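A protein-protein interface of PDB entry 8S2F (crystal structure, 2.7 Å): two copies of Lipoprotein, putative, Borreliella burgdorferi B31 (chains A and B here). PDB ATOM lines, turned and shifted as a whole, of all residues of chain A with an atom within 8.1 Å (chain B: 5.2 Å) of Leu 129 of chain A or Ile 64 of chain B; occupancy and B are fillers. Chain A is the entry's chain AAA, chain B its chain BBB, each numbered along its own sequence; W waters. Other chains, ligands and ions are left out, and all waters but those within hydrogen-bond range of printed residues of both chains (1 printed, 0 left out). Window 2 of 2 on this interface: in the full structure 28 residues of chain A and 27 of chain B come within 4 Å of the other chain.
No position is printed for both chains.
Water W1 bridges O of Met 67 of chain B (3.1 Å) and O of Leu 129 of chain A (3.5 Å).
Lys 122 of chain A touches Gln 60 of chain B (CB to NE2, 3.8 Å). Glu 123 of chain A touches Gln 60 of chain B. NZ of Lys 63 of chain B touches CD1 of Ile 126 of chain A, 3.8 Å away. CD1 of Leu 129 of chain A touches CG2 of Ile 64 of chain B, at 3.9 Å.
The side-chain amino group (NZ) of Lys 122 of chain A sits at hydrogen-bond distance from the side-chain amide oxygen (OD1) of Asn 61 of chain B (2.8 Å).
Of chain B, only Ile 64 comes within 4 Å of Leu 129 of chain A. Of chain A, only Leu 129 (3.9 Å) comes within 4 Å of Ile 64 of chain B. Of the printed residues of chain B, Ile 126 of chain A touches Lys 63 (3.8 Å). Of the printed residues of chain B, Lys 122 of chain A touches Gln 60 and Asn 61. Of the printed residues of chain B, Glu 123 of chain A touches Gln 60. Ser 8 of chain A touches none of the printed residues of chain B. The nearest printed residue of chain A that does not touch Ile 64 of chain B is Ile 125 of chain A (4.1 Å). The nearest printed residue of chain A that does not touch Gln 60 of chain B is Ile 126 of chain A (4.1 Å).
Of the 18 printed residues of chain A, 4 touch a printed residue of chain B. Printed residues of chain A that touch a printed residue of chain B: Lys 122, Glu 123, Ile 126 and Leu 129. Hydrophobic or aromatic side chains of chain A that line the printed part of chain B: Ile 126 and Leu 129. Of the 9 printed residues of chain B, 4 touch a printed residue of chain A.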
ATOM      1  N   PHE A   6       8.278   8.425  10.887  1.00  0.00           N
ATOM      2  CA  PHE A   6       9.203   7.328  11.368  1.00  0.00           C
ATOM      3  C   PHE A   6       9.878   7.721  12.683  1.00  0.00           C
ATOM      4  O   PHE A   6      10.039   8.908  12.955  1.00  0.00           O
ATOM      5  CB  PHE A   6      10.296   7.005  10.341  1.00  0.00           C
ATOM      6  CG  PHE A   6      10.040   5.808   9.455  1.00  0.00           C
ATOM      7  CD1 PHE A   6       9.558   4.610   9.971  1.00  0.00           C
ATOM      8  CD2 PHE A   6      10.323   5.865   8.096  1.00  0.00           C
ATOM      9  CE1 PHE A   6       9.342   3.509   9.153  1.00  0.00           C
ATOM     10  CE2 PHE A   6      10.099   4.766   7.276  1.00  0.00           C
ATOM     11  CZ  PHE A   6       9.616   3.588   7.805  1.00  0.00           C
ATOM     12  N   PRO A   7      10.311   6.747  13.529  1.00  0.00           N
ATOM     13  CA  PRO A   7      10.993   7.050  14.794  1.00  0.00           C
ATOM     14  C   PRO A   7      12.297   7.853  14.609  1.00  0.00           C
ATOM     15  O   PRO A   7      13.241   7.365  13.967  1.00  0.00           O
ATOM     16  CB  PRO A   7      11.284   5.672  15.423  1.00  0.00           C
ATOM     17  CG  PRO A   7      10.318   4.726  14.737  1.00  0.00           C
ATOM     18  CD  PRO A   7      10.126   5.296  13.344  1.00  0.00           C
ATOM     19  N   SER A   8      12.318   9.062  15.187  1.00  0.00           N
ATOM     20  CA  SER A   8      13.367  10.095  14.994  1.00  0.00           C
ATOM     21  C   SER A   8      13.898  10.542  16.355  1.00  0.00           C
ATOM     22  O   SER A   8      15.057  10.236  16.670  1.00  0.00           O
ATOM     23  CB  SER A   8      12.837  11.242  14.189  1.00  0.00           C
ATOM     24  OG  SER A   8      12.612  10.828  12.853  1.00  0.00           O
ATOM     25  N   GLU A  12      12.297   7.842  20.942  1.00  0.00           N
ATOM     26  CA  GLU A  12      11.401   7.013  20.113  1.00  0.00           C
ATOM     27  C   GLU A  12      12.183   5.798  19.635  1.00  0.00           C
ATOM     28  O   GLU A  12      11.643   4.694  19.688  1.00  0.00           O
ATOM     29  CB  GLU A  12      10.913   7.846  18.930  1.00  0.00           C
ATOM     30  CG  GLU A  12       9.920   8.925  19.308  1.00  0.00           C
ATOM     31  CD  GLU A  12       9.533   9.846  18.167  1.00  0.00           C
ATOM     32  OE1 GLU A  12      10.016   9.621  17.043  1.00  0.00           O
ATOM     33  OE2 GLU A  12       8.752  10.784  18.406  1.00  0.00           O
ATOM     34  N   LEU A 121       4.117   4.529  21.401  1.00  0.00           N
ATOM     35  CA  LEU A 121       5.156   5.059  20.486  1.00  0.00           C
ATOM     36  C   LEU A 121       4.437   5.778  19.335  1.00  0.00           C
ATOM     37  O   LEU A 121       4.859   6.892  18.944  1.00  0.00           O
ATOM     38  CB  LEU A 121       6.029   3.895  19.995  1.00  0.00           C
ATOM     39  CG  LEU A 121       6.995   4.187  18.835  1.00  0.00           C
ATOM     40  CD1 LEU A 121       8.236   4.910  19.323  1.00  0.00           C
ATOM     41  CD2 LEU A 121       7.423   2.921  18.113  1.00  0.00           C
ATOM     42  N   LYS A 122       3.357   5.197  18.829  1.00  0.00           N
ATOM     43  CA  LYS A 122       2.712   5.714  17.604  1.00  0.00           C
ATOM     44  C   LYS A 122       1.937   6.979  17.949  1.00  0.00           C
ATOM     45  O   LYS A 122       2.083   7.957  17.219  1.00  0.00           O
ATOM     46  CB  LYS A 122       1.881   4.623  16.934  1.00  0.00           C
ATOM     47  CG  LYS A 122       2.720   3.689  16.076  1.00  0.00           C
ATOM     48  CD  LYS A 122       1.935   2.553  15.497  1.00  0.00           C
ATOM     49  CE  LYS A 122       2.815   1.491  14.870  1.00  0.00           C
ATOM     50  NZ  LYS A 122       3.871   2.076  14.016  1.00  0.00           N
ATOM     51  N   GLU A 123       1.186   6.992  19.040  1.00  0.00           N
ATOM     52  CA  GLU A 123       0.578   8.254  19.539  1.00  0.00           C
ATOM     53  C   GLU A 123       1.703   9.288  19.666  1.00  0.00           C
ATOM     54  O   GLU A 123       1.496  10.443  19.252  1.00  0.00           O
ATOM     55  CB  GLU A 123      -0.138   8.045  20.876  1.00  0.00           C
ATOM     56  CG  GLU A 123      -1.394   7.178  20.802  1.00  0.00           C
ATOM     57  CD  GLU A 123      -1.918   6.740  22.170  1.00  0.00           C
ATOM     58  OE1 GLU A 123      -2.480   5.612  22.279  1.00  0.00           O
ATOM     59  OE2 GLU A 123      -1.764   7.529  23.140  1.00  0.00           O
ATOM     60  N   GLY A 124       2.861   8.867  20.196  1.00  0.00           N
ATOM     61  CA  GLY A 124       4.053   9.710  20.394  1.00  0.00           C
ATOM     62  C   GLY A 124       4.448  10.401  19.104  1.00  0.00           C
ATOM     63  O   GLY A 124       4.687  11.633  19.132  1.00  0.00           O
ATOM     64  N   ILE A 125       4.515   9.639  18.009  1.00  0.00           N
ATOM     65  CA  ILE A 125       4.928  10.130  16.662  1.00  0.00           C
ATOM     66  C   ILE A 125       3.829  11.031  16.073  1.00  0.00           C
ATOM     67  O   ILE A 125       4.177  12.018  15.401  1.00  0.00           O
ATOM     68  CB  ILE A 125       5.268   8.938  15.752  1.00  0.00           C
ATOM     69  CG1 ILE A 125       6.564   8.267  16.215  1.00  0.00           C
ATOM     70  CG2 ILE A 125       5.339   9.369  14.301  1.00  0.00           C
ATOM     71  CD1 ILE A 125       6.718   6.821  15.794  1.00  0.00           C
ATOM     72  N   ILE A 126       2.551  10.726  16.301  1.00  0.00           N
ATOM     73  CA  ILE A 126       1.438  11.602  15.835  1.00  0.00           C
ATOM     74  C   ILE A 126       1.573  12.951  16.548  1.00  0.00           C
ATOM     75  O   ILE A 126       1.507  13.983  15.861  1.00  0.00           O
ATOM     76  CB  ILE A 126       0.059  10.933  16.030  1.00  0.00           C
ATOM     77  CG1 ILE A 126      -0.280  10.018  14.849  1.00  0.00           C
ATOM     78  CG2 ILE A 126      -1.034  11.951  16.248  1.00  0.00           C
ATOM     79  CD1 ILE A 126      -1.227   8.909  15.179  1.00  0.00           C
ATOM     80  N   LYS A 127       1.840  12.941  17.854  1.00  0.00           N
ATOM     81  CA  LYS A 127       1.933  14.173  18.687  1.00  0.00           C
ATOM     82  C   LYS A 127       3.035  15.103  18.149  1.00  0.00           C
ATOM     83  O   LYS A 127       2.829  16.327  18.150  1.00  0.00           O
ATOM     84  CB  LYS A 127       2.147  13.802  20.160  1.00  0.00           C
ATOM     85  CG  LYS A 127       1.093  14.353  21.113  1.00  0.00           C
ATOM     86  CD  LYS A 127      -0.296  13.750  20.926  1.00  0.00           C
ATOM     87  CE  LYS A 127      -1.436  14.673  21.315  1.00  0.00           C
ATOM     88  NZ  LYS A 127      -1.425  15.935  20.532  1.00  0.00           N
ATOM     89  N   ARG A 128       4.155  14.545  17.682  1.00  0.00           N
ATOM     90  CA  ARG A 128       5.302  15.313  17.128  1.00  0.00           C
ATOM     91  C   ARG A 128       4.965  15.819  15.719  1.00  0.00           C
ATOM     92  O   ARG A 128       5.400  16.936  15.383  1.00  0.00           O
ATOM     93  CB  ARG A 128       6.582  14.466  17.128  1.00  0.00           C
ATOM     94  CG  ARG A 128       7.590  14.849  16.052  1.00  0.00           C
ATOM     95  CD  ARG A 128       8.955  14.218  16.228  1.00  0.00           C
ATOM     96  NE  ARG A 128       8.959  12.787  15.957  1.00  0.00           N
ATOM     97  CZ  ARG A 128       8.884  12.243  14.747  1.00  0.00           C
ATOM     98  NH1 ARG A 128       8.791  13.004  13.668  1.00  0.00           N
ATOM     99  NH2 ARG A 128       8.903  10.928  14.614  1.00  0.00           N
ATOM    100  N   LEU A 129       4.257  15.025  14.909  1.00  0.00           N
ATOM    101  CA  LEU A 129       3.923  15.388  13.507  1.00  0.00           C
ATOM    102  C   LEU A 129       2.998  16.609  13.561  1.00  0.00           C
ATOM    103  O   LEU A 129       3.096  17.491  12.684  1.00  0.00           O
ATOM    104  CB  LEU A 129       3.403  14.144  12.781  1.00  0.00           C
ATOM    105  CG  LEU A 129       4.463  13.067  12.540  1.00  0.00           C
ATOM    106  CD1 LEU A 129       3.847  11.788  12.004  1.00  0.00           C
ATOM    107  CD2 LEU A 129       5.557  13.562  11.604  1.00  0.00           C
ATOM    108  N   GLU A 130       2.308  16.741  14.685  1.00  0.00           N
ATOM    109  CA  GLU A 130       1.332  17.836  14.856  1.00  0.00           C
ATOM    110  C   GLU A 130       1.985  19.104  15.405  1.00  0.00           C
ATOM    111  O   GLU A 130       1.319  20.148  15.355  1.00  0.00           O
ATOM    112  CB  GLU A 130       0.340  17.414  15.932  1.00  0.00           C
ATOM    113  CG  GLU A 130      -0.544  16.261  15.506  1.00  0.00           C
ATOM    114  CD  GLU A 130      -1.510  15.787  16.576  1.00  0.00           C
ATOM    115  OE1 GLU A 130      -2.530  15.177  16.217  1.00  0.00           O
ATOM    116  OE2 GLU A 130      -1.238  16.034  17.763  1.00  0.00           O
ATOM    117  N   LYS A 131       3.227  19.021  15.896  1.00  0.00           N
ATOM    118  CA  LYS A 131       3.975  20.192  16.448  1.00  0.00           C
ATOM    119  C   LYS A 131       3.290  20.662  17.733  1.00  0.00           C
ATOM    120  O   LYS A 131       3.442  21.838  18.098  1.00  0.00           O
ATOM    121  CB  LYS A 131       4.072  21.281  15.374  1.00  0.00           C
ATOM    122  CG  LYS A 131       5.222  21.122  14.391  1.00  0.00           C
ATOM    123  CD  LYS A 131       5.101  19.892  13.521  1.00  0.00           C
ATOM    124  CE  LYS A 131       6.006  19.928  12.308  1.00  0.00           C
ATOM    125  NZ  LYS A 131       5.419  20.731  11.210  1.00  0.00           N
ATOM    126  N   SER A 132       2.582  19.751  18.385  1.00  0.00           N
ATOM    127  CA  SER A 132       1.871  20.018  19.668  1.00  0.00           C
ATOM    128  C   SER A 132       2.841  19.714  20.823  1.00  0.00           C
ATOM    129  O   SER A 132       2.486  18.917  21.721  1.00  0.00           O
ATOM    130  CB  SER A 132       0.595  19.209  19.776  1.00  0.00           C
ATOM    131  OG  SER A 132       0.861  17.817  19.650  1.00  0.00           O
ATOM    132  N   LYS A 133       4.007  20.373  20.813  1.00  0.00           N
ATOM    133  CA  LYS A 133       5.207  19.990  21.606  1.00  0.00           C
ATOM    134  C   LYS A 133       5.288  20.805  22.896  1.00  0.00           C
ATOM    135  O   LYS A 133       5.990  21.834  22.904  1.00  0.00           O
ATOM    136  CB  LYS A 133       6.498  20.233  20.814  1.00  0.00           C
ATOM    137  CG  LYS A 133       6.456  19.846  19.344  1.00  0.00           C
ATOM    138  CD  LYS A 133       6.147  18.381  19.102  1.00  0.00           C
ATOM    139  CE  LYS A 133       7.374  17.489  19.134  1.00  0.00           C
ATOM    140  NZ  LYS A 133       7.882  17.277  20.511  1.00  0.00           N
ATOM    141  N   ALA A 137       4.694  14.759  23.161  1.00  0.00           N
ATOM    142  CA  ALA A 137       5.357  13.823  22.217  1.00  0.00           C
ATOM    143  C   ALA A 137       6.298  12.870  22.973  1.00  0.00           C
ATOM    144  O   ALA A 137       6.108  11.645  22.874  1.00  0.00           O
ATOM    145  CB  ALA A 137       6.105  14.609  21.172  1.00  0.00           C
ATOM    146  N   GLN B  60      -3.235   3.332  13.026  1.00  0.00           N
ATOM    147  CA  GLN B  60      -2.311   4.349  13.589  1.00  0.00           C
ATOM    148  C   GLN B  60      -1.254   4.675  12.539  1.00  0.00           C
ATOM    149  O   GLN B  60      -0.854   5.830  12.469  1.00  0.00           O
ATOM    150  CB  GLN B  60      -1.670   3.856  14.888  1.00  0.00           C
ATOM    151  CG  GLN B  60      -2.559   3.998  16.125  1.00  0.00           C
ATOM    152  CD  GLN B  60      -1.786   3.623  17.368  1.00  0.00           C
ATOM    153  OE1 GLN B  60      -1.283   2.507  17.498  1.00  0.00           O
ATOM    154  NE2 GLN B  60      -1.637   4.565  18.285  1.00  0.00           N
ATOM    155  N   ASN B  61      -0.867   3.680  11.737  1.00  0.00           N
ATOM    156  CA  ASN B  61       0.025   3.839  10.560  1.00  0.00           C
ATOM    157  C   ASN B  61      -0.679   4.643   9.455  1.00  0.00           C
ATOM    158  O   ASN B  61      -0.020   5.470   8.831  1.00  0.00           O
ATOM    159  CB  ASN B  61       0.508   2.475  10.076  1.00  0.00           C
ATOM    160  CG  ASN B  61       1.533   1.854  11.004  1.00  0.00           C
ATOM    161  OD1 ASN B  61       2.145   2.542  11.813  1.00  0.00           O
ATOM    162  ND2 ASN B  61       1.725   0.548  10.901  1.00  0.00           N
ATOM    163  N   LYS B  62      -1.975   4.440   9.218  1.00  0.00           N
ATOM    164  CA  LYS B  62      -2.721   5.257   8.231  1.00  0.00           C
ATOM    165  C   LYS B  62      -2.704   6.710   8.688  1.00  0.00           C
ATOM    166  O   LYS B  62      -2.465   7.579   7.828  1.00  0.00           O
ATOM    167  CB  LYS B  62      -4.155   4.779   7.988  1.00  0.00           C
ATOM    168  CG  LYS B  62      -4.399   4.149   6.620  1.00  0.00           C
ATOM    169  CD  LYS B  62      -3.902   5.012   5.463  1.00  0.00           C
ATOM    170  CE  LYS B  62      -4.493   4.645   4.117  1.00  0.00           C
ATOM    171  NZ  LYS B  62      -4.500   5.806   3.192  1.00  0.00           N
ATOM    172  N   LYS B  63      -2.924   6.985   9.974  1.00  0.00           N
ATOM    173  CA  LYS B  63      -2.929   8.394  10.454  1.00  0.00           C
ATOM    174  C   LYS B  63      -1.577   9.032  10.110  1.00  0.00           C
ATOM    175  O   LYS B  63      -1.597  10.071   9.435  1.00  0.00           O
ATOM    176  CB  LYS B  63      -3.285   8.504  11.941  1.00  0.00           C
ATOM    177  CG  LYS B  63      -4.767   8.288  12.234  1.00  0.00           C
ATOM    178  CD  LYS B  63      -5.235   8.816  13.577  1.00  0.00           C
ATOM    179  CE  LYS B  63      -5.041   7.832  14.711  1.00  0.00           C
ATOM    180  NZ  LYS B  63      -4.939   8.536  16.011  1.00  0.00           N
ATOM    181  N   ILE B  64      -0.467   8.399  10.522  1.00  0.00           N
ATOM    182  CA  ILE B  64       0.937   8.874  10.311  1.00  0.00           C
ATOM    183  C   ILE B  64       1.094   9.156   8.817  1.00  0.00           C
ATOM    184  O   ILE B  64       1.549  10.256   8.456  1.00  0.00           O
ATOM    185  CB  ILE B  64       1.987   7.858  10.830  1.00  0.00           C
ATOM    186  CG1 ILE B  64       1.918   7.671  12.345  1.00  0.00           C
ATOM    187  CG2 ILE B  64       3.409   8.246  10.418  1.00  0.00           C
ATOM    188  CD1 ILE B  64       2.777   6.547  12.863  1.00  0.00           C
ATOM    189  N   SER B  65       0.710   8.189   7.987  1.00  0.00           N
ATOM    190  CA  SER B  65       0.728   8.266   6.502  1.00  0.00           C
ATOM    191  C   SER B  65      -0.007   9.527   6.005  1.00  0.00           C
ATOM    192  O   SER B  65       0.592  10.282   5.276  1.00  0.00           O
ATOM    193  CB  SER B  65       0.164   6.986   5.952  1.00  0.00           C
ATOM    194  OG  SER B  65      -0.020   7.082   4.563  1.00  0.00           O
ATOM    195  N   LEU B  66      -1.247   9.767   6.432  1.00  0.00           N
ATOM    196  CA  LEU B  66      -2.073  10.940   6.021  1.00  0.00           C
ATOM    197  C   LEU B  66      -1.547  12.242   6.640  1.00  0.00           C
ATOM    198  O   LEU B  66      -1.906  13.318   6.119  1.00  0.00           O
ATOM    199  CB  LEU B  66      -3.531  10.746   6.454  1.00  0.00           C
ATOM    200  CG  LEU B  66      -4.285   9.585   5.801  1.00  0.00           C
ATOM    201  CD1 LEU B  66      -5.653   9.376   6.459  1.00  0.00           C
ATOM    202  CD2 LEU B  66      -4.423   9.794   4.304  1.00  0.00           C
ATOM    203  N   MET B  67      -0.771  12.162   7.720  1.00  0.00           N
ATOM    204  CA  MET B  67      -0.326  13.347   8.506  1.00  0.00           C
ATOM    205  C   MET B  67       0.666  14.179   7.690  1.00  0.00           C
ATOM    206  O   MET B  67       0.743  15.387   7.934  1.00  0.00           O
ATOM    207  CB  MET B  67       0.350  12.924   9.810  1.00  0.00           C
ATOM    208  CG  MET B  67      -0.584  12.264  10.788  1.00  0.00           C
ATOM    209  SD  MET B  67      -0.867  13.361  12.144  1.00  0.00           S
ATOM    210  CE  MET B  67      -1.963  14.516  11.323  1.00  0.00           C
ATOM    211  N   LYS B  68       1.400  13.553   6.769  1.00  0.00           N
ATOM    212  CA  LYS B  68       2.282  14.248   5.794  1.00  0.00           C
ATOM    213  C   LYS B  68       1.525  15.440   5.196  1.00  0.00           C
ATOM    214  O   LYS B  68       2.167  16.471   4.964  1.00  0.00           O
ATOM    215  CB  LYS B  68       2.751  13.272   4.712  1.00  0.00           C
ATOM    216  CG  LYS B  68       3.450  13.923   3.531  1.00  0.00           C
ATOM    217  CD  LYS B  68       4.493  13.051   2.881  1.00  0.00           C
ATOM    218  CE  LYS B  68       5.611  13.872   2.276  1.00  0.00           C
ATOM    219  NZ  LYS B  68       6.814  13.046   2.023  1.00  0.00           N
HETATM  220  O   HOH W   1       3.074  16.956   9.240  1.00  0.00           O
